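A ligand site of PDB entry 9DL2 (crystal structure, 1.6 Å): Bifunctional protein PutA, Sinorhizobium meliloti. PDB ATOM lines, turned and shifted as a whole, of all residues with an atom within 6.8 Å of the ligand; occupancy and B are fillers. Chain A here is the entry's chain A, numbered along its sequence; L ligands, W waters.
An oxygen (O3) of the ligand is in hydrogen-bond range of the side-chain hydroxyl of Ser 847 (2.8 Å).
NH1 of Arg 845 lies within salt-bridge range of O3 of the ligand (2.9 Å).
An oxygen (O4) of the ligand is in hydrogen-bond range of the backbone NH (N) of Ala 1005 (2.9 Å).
The backbone NH (N) of Gly 1004 sits at hydrogen-bond distance from an oxygen (O4) of the ligand (3.1 Å).
O of Ser 847 is in hydrogen-bond range of OG1 of Thr 973.
NH2 of Arg 845 lies within hydrogen-bond range of OD1 of Asn 669 (3.3 Å).
The backbone NH (N) of Phe 1012 lies within hydrogen-bond range of the backbone carbonyl oxygen (O) of Ala 1024, 2.9 Å away.
N of Ala 713 is in hydrogen-bond range of OE2 of Glu 673, 2.7 Å away.
OE1 of Glu 673 is in salt-bridge range of NZ of Lys 665, 3.0 Å away.
Residues that only touch the ligand: Glu 673 (3.8 Å), Glu 676 (3.3 Å), Phe 710 (3.5 Å), Ala 713 (3.6 Å), Ile 1003 (3.8 Å) and Phe 1012 (3.5 Å).
Hydrophobic or aromatic side chains within 4 Å of the ligand: Phe 710, Ala 713, Ala 1005 and Phe 1012.
Ten residues have an atom within 4 Å of the ligand: Glu 673, Glu 676, Phe 710, Ala 713, Arg 845, Ser 847, Ile 1003, Gly 1004, Ala 1005 and Phe 1012.
The nearest printed residue that does not touch the ligand is Ile 714 (4.04 Å).
Water W1 lies within hydrogen-bond range of OH of Tyr 997, O of Ile 1002 and O4 of the ligand.
Water W3 lies within hydrogen-bond range of the guanidinium group (NH1) of Arg 845 and an oxygen (O1) of the ligand.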
ATOM      1  N   LYS A 665      -7.832  -0.702  11.629  1.00  0.00           N
ATOM      2  CA  LYS A 665      -7.153  -0.280  10.414  1.00  0.00           C
ATOM      3  C   LYS A 665      -5.901  -1.093  10.152  1.00  0.00           C
ATOM      4  O   LYS A 665      -5.240  -1.569  11.075  1.00  0.00           O
ATOM      5  CB  LYS A 665      -6.772   1.182  10.499  1.00  0.00           C
ATOM      6  CG  LYS A 665      -7.974   2.055  10.690  1.00  0.00           C
ATOM      7  CD  LYS A 665      -7.766   3.346   9.969  1.00  0.00           C
ATOM      8  CE  LYS A 665      -9.057   4.095   9.920  1.00  0.00           C
ATOM      9  NZ  LYS A 665      -8.876   5.346   9.133  1.00  0.00           N
ATOM     10  N   ASN A 669      -3.003   1.932   6.162  1.00  0.00           N
ATOM     11  CA  ASN A 669      -4.017   2.966   6.374  1.00  0.00           C
ATOM     12  C   ASN A 669      -3.752   3.782   7.629  1.00  0.00           C
ATOM     13  O   ASN A 669      -4.034   4.984   7.650  1.00  0.00           O
ATOM     14  CB  ASN A 669      -5.397   2.324   6.442  1.00  0.00           C
ATOM     15  CG  ASN A 669      -5.823   1.701   5.118  1.00  0.00           C
ATOM     16  OD1 ASN A 669      -5.407   2.151   4.040  1.00  0.00           O
ATOM     17  ND2 ASN A 669      -6.663   0.684   5.182  1.00  0.00           N
ATOM     18  N   ALA A 672      -1.188   6.476   6.757  1.00  0.00           N
ATOM     19  CA  ALA A 672      -1.779   7.575   6.025  1.00  0.00           C
ATOM     20  C   ALA A 672      -2.656   8.417   6.932  1.00  0.00           C
ATOM     21  O   ALA A 672      -2.708   9.643   6.777  1.00  0.00           O
ATOM     22  CB  ALA A 672      -2.568   7.042   4.830  1.00  0.00           C
ATOM     23  N   GLU A 673      -3.313   7.787   7.903  1.00  0.00           N
ATOM     24  CA  GLU A 673      -4.127   8.512   8.872  1.00  0.00           C
ATOM     25  C   GLU A 673      -3.271   9.460   9.710  1.00  0.00           C
ATOM     26  O   GLU A 673      -3.624  10.629   9.909  1.00  0.00           O
ATOM     27  CB  GLU A 673      -4.862   7.506   9.760  1.00  0.00           C
ATOM     28  CG  GLU A 673      -5.646   8.134  10.869  1.00  0.00           C
ATOM     29  CD  GLU A 673      -7.081   8.415  10.483  1.00  0.00           C
ATOM     30  OE1 GLU A 673      -7.504   7.975   9.390  1.00  0.00           O
ATOM     31  OE2 GLU A 673      -7.779   9.057  11.280  1.00  0.00           O
ATOM     32  N   VAL A 674      -2.151   8.964  10.228  1.00  0.00           N
ATOM     33  CA  VAL A 674      -1.293   9.838  11.030  1.00  0.00           C
ATOM     34  C   VAL A 674      -0.696  10.926  10.163  1.00  0.00           C
ATOM     35  O   VAL A 674      -0.600  12.085  10.574  1.00  0.00           O
ATOM     36  CB  VAL A 674      -0.207   9.023  11.756  1.00  0.00           C
ATOM     37  CG1 VAL A 674       0.694   9.954  12.560  1.00  0.00           C
ATOM     38  CG2 VAL A 674      -0.837   7.965  12.693  1.00  0.00           C
ATOM     39  N   GLU A 676      -2.100  12.296   7.612  1.00  0.00           N
ATOM     40  CA  GLU A 676      -3.142  13.282   7.392  1.00  0.00           C
ATOM     41  C   GLU A 676      -3.290  14.213   8.589  1.00  0.00           C
ATOM     42  O   GLU A 676      -3.482  15.417   8.426  1.00  0.00           O
ATOM     43  CB  GLU A 676      -4.475  12.596   7.109  1.00  0.00           C
ATOM     44  CG  GLU A 676      -5.521  13.538   6.546  1.00  0.00           C
ATOM     45  CD  GLU A 676      -5.636  13.424   5.036  1.00  0.00           C
ATOM     46  OE1 GLU A 676      -4.730  12.805   4.426  1.00  0.00           O
ATOM     47  OE2 GLU A 676      -6.610  13.932   4.460  1.00  0.00           O
ATOM     48  N   ALA A 677      -3.205  13.662   9.796  1.00  0.00           N
ATOM     49  CA  ALA A 677      -3.301  14.505  10.979  1.00  0.00           C
ATOM     50  C   ALA A 677      -2.147  15.494  11.020  1.00  0.00           C
ATOM     51  O   ALA A 677      -2.346  16.686  11.296  1.00  0.00           O
ATOM     52  CB  ALA A 677      -3.321  13.645  12.244  1.00  0.00           C
ATOM     53  N   PHE A 680      -2.866  18.153   8.369  1.00  0.00           N
ATOM     54  CA  PHE A 680      -3.855  19.108   8.865  1.00  0.00           C
ATOM     55  C   PHE A 680      -3.217  20.140   9.773  1.00  0.00           C
ATOM     56  O   PHE A 680      -3.437  21.347   9.612  1.00  0.00           O
ATOM     57  CB  PHE A 680      -4.979  18.403   9.633  1.00  0.00           C
ATOM     58  CG  PHE A 680      -6.090  17.886   8.772  1.00  0.00           C
ATOM     59  CD1 PHE A 680      -6.693  18.682   7.816  1.00  0.00           C
ATOM     60  CD2 PHE A 680      -6.541  16.587   8.932  1.00  0.00           C
ATOM     61  CE1 PHE A 680      -7.733  18.204   7.049  1.00  0.00           C
ATOM     62  CE2 PHE A 680      -7.570  16.090   8.163  1.00  0.00           C
ATOM     63  CZ  PHE A 680      -8.171  16.891   7.215  1.00  0.00           C
ATOM     64  N   PHE A 710     -12.053   7.872  10.742  1.00  0.00           N
ATOM     65  CA  PHE A 710     -10.765   8.567  10.693  1.00  0.00           C
ATOM     66  C   PHE A 710     -10.541   9.138  12.074  1.00  0.00           C
ATOM     67  O   PHE A 710     -10.615  10.351  12.290  1.00  0.00           O
ATOM     68  CB  PHE A 710     -10.733   9.657   9.616  1.00  0.00           C
ATOM     69  CG  PHE A 710     -10.927   9.129   8.201  1.00  0.00           C
ATOM     70  CD1 PHE A 710     -10.246   8.020   7.762  1.00  0.00           C
ATOM     71  CD2 PHE A 710     -11.798   9.776   7.327  1.00  0.00           C
ATOM     72  CE1 PHE A 710     -10.421   7.550   6.463  1.00  0.00           C
ATOM     73  CE2 PHE A 710     -11.971   9.323   6.029  1.00  0.00           C
ATOM     74  CZ  PHE A 710     -11.284   8.195   5.601  1.00  0.00           C
ATOM     75  N   ALA A 713      -7.260  11.561  12.201  1.00  0.00           N
ATOM     76  CA  ALA A 713      -7.038  12.611  11.211  1.00  0.00           C
ATOM     77  C   ALA A 713      -8.167  13.634  11.223  1.00  0.00           C
ATOM     78  O   ALA A 713      -7.915  14.837  11.338  1.00  0.00           O
ATOM     79  CB  ALA A 713      -6.883  11.984   9.832  1.00  0.00           C
ATOM     80  N   ILE A 714      -9.412  13.186  11.084  1.00  0.00           N
ATOM     81  CA  ILE A 714     -10.507  14.159  11.074  1.00  0.00           C
ATOM     82  C   ILE A 714     -10.685  14.777  12.450  1.00  0.00           C
ATOM     83  O   ILE A 714     -10.954  15.985  12.585  1.00  0.00           O
ATOM     84  CB  ILE A 714     -11.796  13.487  10.570  1.00  0.00           C
ATOM     85  CG1 ILE A 714     -11.616  13.199   9.080  1.00  0.00           C
ATOM     86  CG2 ILE A 714     -13.026  14.395  10.864  1.00  0.00           C
ATOM     87  CD1 ILE A 714     -12.869  12.852   8.377  1.00  0.00           C
ATOM     88  N   ARG A 845     -14.612   4.438   4.483  1.00  0.00           N
ATOM     89  CA  ARG A 845     -14.199   5.790   4.164  1.00  0.00           C
ATOM     90  C   ARG A 845     -15.413   6.521   3.622  1.00  0.00           C
ATOM     91  O   ARG A 845     -16.205   5.933   2.892  1.00  0.00           O
ATOM     92  CB  ARG A 845     -13.099   5.799   3.110  1.00  0.00           C
ATOM     93  CG  ARG A 845     -11.810   5.161   3.568  1.00  0.00           C
ATOM     94  CD  ARG A 845     -10.796   5.325   2.457  1.00  0.00           C
ATOM     95  NE  ARG A 845      -9.516   4.710   2.794  1.00  0.00           N
ATOM     96  CZ  ARG A 845      -8.436   5.393   3.125  1.00  0.00           C
ATOM     97  NH1 ARG A 845      -8.433   6.713   3.187  1.00  0.00           N
ATOM     98  NH2 ARG A 845      -7.308   4.721   3.370  1.00  0.00           N
ATOM     99  N   CYS A 846     -15.546   7.801   3.950  1.00  0.00           N
ATOM    100  CA  CYS A 846     -16.636   8.547   3.340  1.00  0.00           C
ATOM    101  C   CYS A 846     -16.469   8.618   1.830  1.00  0.00           C
ATOM    102  O   CYS A 846     -17.450   8.684   1.103  1.00  0.00           O
ATOM    103  CB  CYS A 846     -16.672   9.957   3.904  1.00  0.00           C
ATOM    104  SG  CYS A 846     -15.037  10.690   3.911  1.00  0.00           S
ATOM    105  N   SER A 847     -15.225   8.560   1.379  1.00  0.00           N
ATOM    106  CA  SER A 847     -14.832   8.636  -0.021  1.00  0.00           C
ATOM    107  C   SER A 847     -14.944   7.324  -0.763  1.00  0.00           C
ATOM    108  O   SER A 847     -14.680   7.305  -1.971  1.00  0.00           O
ATOM    109  CB  SER A 847     -13.375   9.105  -0.089  1.00  0.00           C
ATOM    110  OG  SER A 847     -12.587   8.245   0.719  1.00  0.00           O
ATOM    111  N   ALA A 848     -15.274   6.232  -0.085  1.00  0.00           N
ATOM    112  CA  ALA A 848     -15.196   4.906  -0.685  1.00  0.00           C
ATOM    113  C   ALA A 848     -16.077   4.794  -1.915  1.00  0.00           C
ATOM    114  O   ALA A 848     -17.158   5.377  -2.005  1.00  0.00           O
ATOM    115  CB  ALA A 848     -15.596   3.832   0.341  1.00  0.00           C
ATOM    116  N   THR A 973     -17.145  12.111  -3.474  1.00  0.00           N
ATOM    117  CA  THR A 973     -16.081  11.747  -4.405  1.00  0.00           C
ATOM    118  C   THR A 973     -16.684  11.145  -5.663  1.00  0.00           C
ATOM    119  O   THR A 973     -17.804  10.641  -5.681  1.00  0.00           O
ATOM    120  CB  THR A 973     -15.077  10.773  -3.791  1.00  0.00           C
ATOM    121  OG1 THR A 973     -15.748   9.580  -3.383  1.00  0.00           O
ATOM    122  CG2 THR A 973     -14.395  11.413  -2.584  1.00  0.00           C
ATOM    123  N   TYR A 997     -11.698  12.478  -9.379  1.00  0.00           N
ATOM    124  CA  TYR A 997     -10.465  11.728  -9.558  1.00  0.00           C
ATOM    125  C   TYR A 997     -10.487  11.118 -10.940  1.00  0.00           C
ATOM    126  O   TYR A 997     -11.454  10.445 -11.297  1.00  0.00           O
ATOM    127  CB  TYR A 997     -10.336  10.624  -8.501  1.00  0.00           C
ATOM    128  CG  TYR A 997     -10.239  11.194  -7.107  1.00  0.00           C
ATOM    129  CD1 TYR A 997      -9.027  11.654  -6.612  1.00  0.00           C
ATOM    130  CD2 TYR A 997     -11.371  11.298  -6.311  1.00  0.00           C
ATOM    131  CE1 TYR A 997      -8.934  12.171  -5.328  1.00  0.00           C
ATOM    132  CE2 TYR A 997     -11.285  11.810  -5.023  1.00  0.00           C
ATOM    133  CZ  TYR A 997     -10.071  12.248  -4.549  1.00  0.00           C
ATOM    134  OH  TYR A 997      -9.970  12.770  -3.270  1.00  0.00           O
ATOM    135  N   ILE A1002     -10.250   6.845  -5.806  1.00  0.00           N
ATOM    136  CA  ILE A1002     -11.017   8.006  -5.360  1.00  0.00           C
ATOM    137  C   ILE A1002     -10.881   8.228  -3.849  1.00  0.00           C
ATOM    138  O   ILE A1002     -11.681   8.968  -3.263  1.00  0.00           O
ATOM    139  CB  ILE A1002     -12.496   7.910  -5.774  1.00  0.00           C
ATOM    140  CG1 ILE A1002     -13.226   6.780  -5.037  1.00  0.00           C
ATOM    141  CG2 ILE A1002     -12.602   7.748  -7.280  1.00  0.00           C
ATOM    142  CD1 ILE A1002     -14.743   6.776  -5.299  1.00  0.00           C
ATOM    143  N   ILE A1003      -9.885   7.633  -3.223  1.00  0.00           N
ATOM    144  CA  ILE A1003      -9.753   7.695  -1.766  1.00  0.00           C
ATOM    145  C   ILE A1003      -8.422   8.337  -1.382  1.00  0.00           C
ATOM    146  O   ILE A1003      -7.549   8.582  -2.209  1.00  0.00           O
ATOM    147  CB  ILE A1003      -9.873   6.308  -1.119  1.00  0.00           C
ATOM    148  CG1 ILE A1003      -8.750   5.369  -1.578  1.00  0.00           C
ATOM    149  CG2 ILE A1003     -11.248   5.719  -1.360  1.00  0.00           C
ATOM    150  CD1 ILE A1003      -8.630   4.104  -0.692  1.00  0.00           C
ATOM    151  N   GLY A1004      -8.275   8.601  -0.092  1.00  0.00           N
ATOM    152  CA  GLY A1004      -7.025   9.120   0.420  1.00  0.00           C
ATOM    153  C   GLY A1004      -6.741  10.551   0.002  1.00  0.00           C
ATOM    154  O   GLY A1004      -5.585  10.878  -0.317  1.00  0.00           O
ATOM    155  N   ALA A1005      -7.749  11.407   0.003  1.00  0.00           N
ATOM    156  CA  ALA A1005      -7.546  12.820  -0.281  1.00  0.00           C
ATOM    157  C   ALA A1005      -6.447  13.372   0.620  1.00  0.00           C
ATOM    158  O   ALA A1005      -6.378  13.045   1.808  1.00  0.00           O
ATOM    159  CB  ALA A1005      -8.836  13.605  -0.065  1.00  0.00           C
ATOM    160  N   VAL A1006      -5.592  14.193   0.031  1.00  0.00           N
ATOM    161  CA  VAL A1006      -4.405  14.732   0.685  1.00  0.00           C
ATOM    162  C   VAL A1006      -4.643  16.182   1.032  1.00  0.00           C
ATOM    163  O   VAL A1006      -5.013  16.984   0.174  1.00  0.00           O
ATOM    164  CB  VAL A1006      -3.160  14.575  -0.206  1.00  0.00           C
ATOM    165  CG1 VAL A1006      -1.964  15.266   0.410  1.00  0.00           C
ATOM    166  CG2 VAL A1006      -2.870  13.107  -0.444  1.00  0.00           C
ATOM    167  N   VAL A1007      -4.415  16.530   2.303  1.00  0.00           N
ATOM    168  CA  VAL A1007      -4.586  17.891   2.790  1.00  0.00           C
ATOM    169  C   VAL A1007      -3.842  18.861   1.899  1.00  0.00           C
ATOM    170  O   VAL A1007      -2.662  18.643   1.585  1.00  0.00           O
ATOM    171  CB  VAL A1007      -4.081  17.973   4.238  1.00  0.00           C
ATOM    172  CG1 VAL A1007      -4.163  19.409   4.734  1.00  0.00           C
ATOM    173  CG2 VAL A1007      -4.890  17.058   5.130  1.00  0.00           C
ATOM    174  N   PHE A1012     -10.799  18.547   0.708  1.00  0.00           N
ATOM    175  CA  PHE A1012     -11.760  17.461   0.718  1.00  0.00           C
ATOM    176  C   PHE A1012     -13.128  17.919   1.214  1.00  0.00           C
ATOM    177  O   PHE A1012     -13.228  18.546   2.284  1.00  0.00           O
ATOM    178  CB  PHE A1012     -11.279  16.289   1.587  1.00  0.00           C
ATOM    179  CG  PHE A1012     -12.180  15.095   1.487  1.00  0.00           C
ATOM    180  CD1 PHE A1012     -12.167  14.284   0.358  1.00  0.00           C
ATOM    181  CD2 PHE A1012     -13.088  14.817   2.508  1.00  0.00           C
ATOM    182  CE1 PHE A1012     -13.017  13.206   0.247  1.00  0.00           C
ATOM    183  CE2 PHE A1012     -13.947  13.722   2.410  1.00  0.00           C
ATOM    184  CZ  PHE A1012     -13.898  12.905   1.290  1.00  0.00           C
ATOM    185  N   ALA A1024     -12.475  20.743   4.217  1.00  0.00           N
ATOM    186  CA  ALA A1024     -11.350  20.499   5.114  1.00  0.00           C
ATOM    187  C   ALA A1024     -10.063  20.387   4.295  1.00  0.00           C
ATOM    188  O   ALA A1024     -10.068  19.881   3.167  1.00  0.00           O
ATOM    189  CB  ALA A1024     -11.584  19.220   5.916  1.00  0.00           C
HETATM  190  C1  LIG L   1      -7.296  10.277   6.366  1.00  0.00           C
HETATM  191  C2  LIG L   1      -7.087   9.825   4.939  1.00  0.00           C
HETATM  192  O1  LIG L   1      -8.286   9.592   4.274  1.00  0.00           O
HETATM  193  C3  LIG L   1      -9.153  10.718   4.341  1.00  0.00           C
HETATM  194  C4  LIG L   1     -10.091  10.954   3.320  1.00  0.00           C
HETATM  195  C5  LIG L   1     -10.923  12.069   3.387  1.00  0.00           C
HETATM  196  C6  LIG L   1     -10.818  12.943   4.468  1.00  0.00           C
HETATM  197  C7  LIG L   1      -9.880  12.725   5.465  1.00  0.00           C
HETATM  198  C8  LIG L   1      -9.049  11.598   5.405  1.00  0.00           C
HETATM  199  O2  LIG L   1      -8.101  11.405   6.469  1.00  0.00           O
HETATM  200  C9  LIG L   1     -10.263  10.036   2.124  1.00  0.00           C
HETATM  201  O3  LIG L   1     -10.275   8.779   2.250  1.00  0.00           O
HETATM  202  O4  LIG L   1     -10.382  10.554   0.981  1.00  0.00           O
HETATM  203  O   HOH W   1     -11.059  11.114  -1.645  1.00  0.00           O
HETATM  204  O   HOH W   2     -11.195  15.744   6.009  1.00  0.00           O
HETATM  205  O   HOH W   3      -5.612   7.655   3.544  1.00  0.00           O
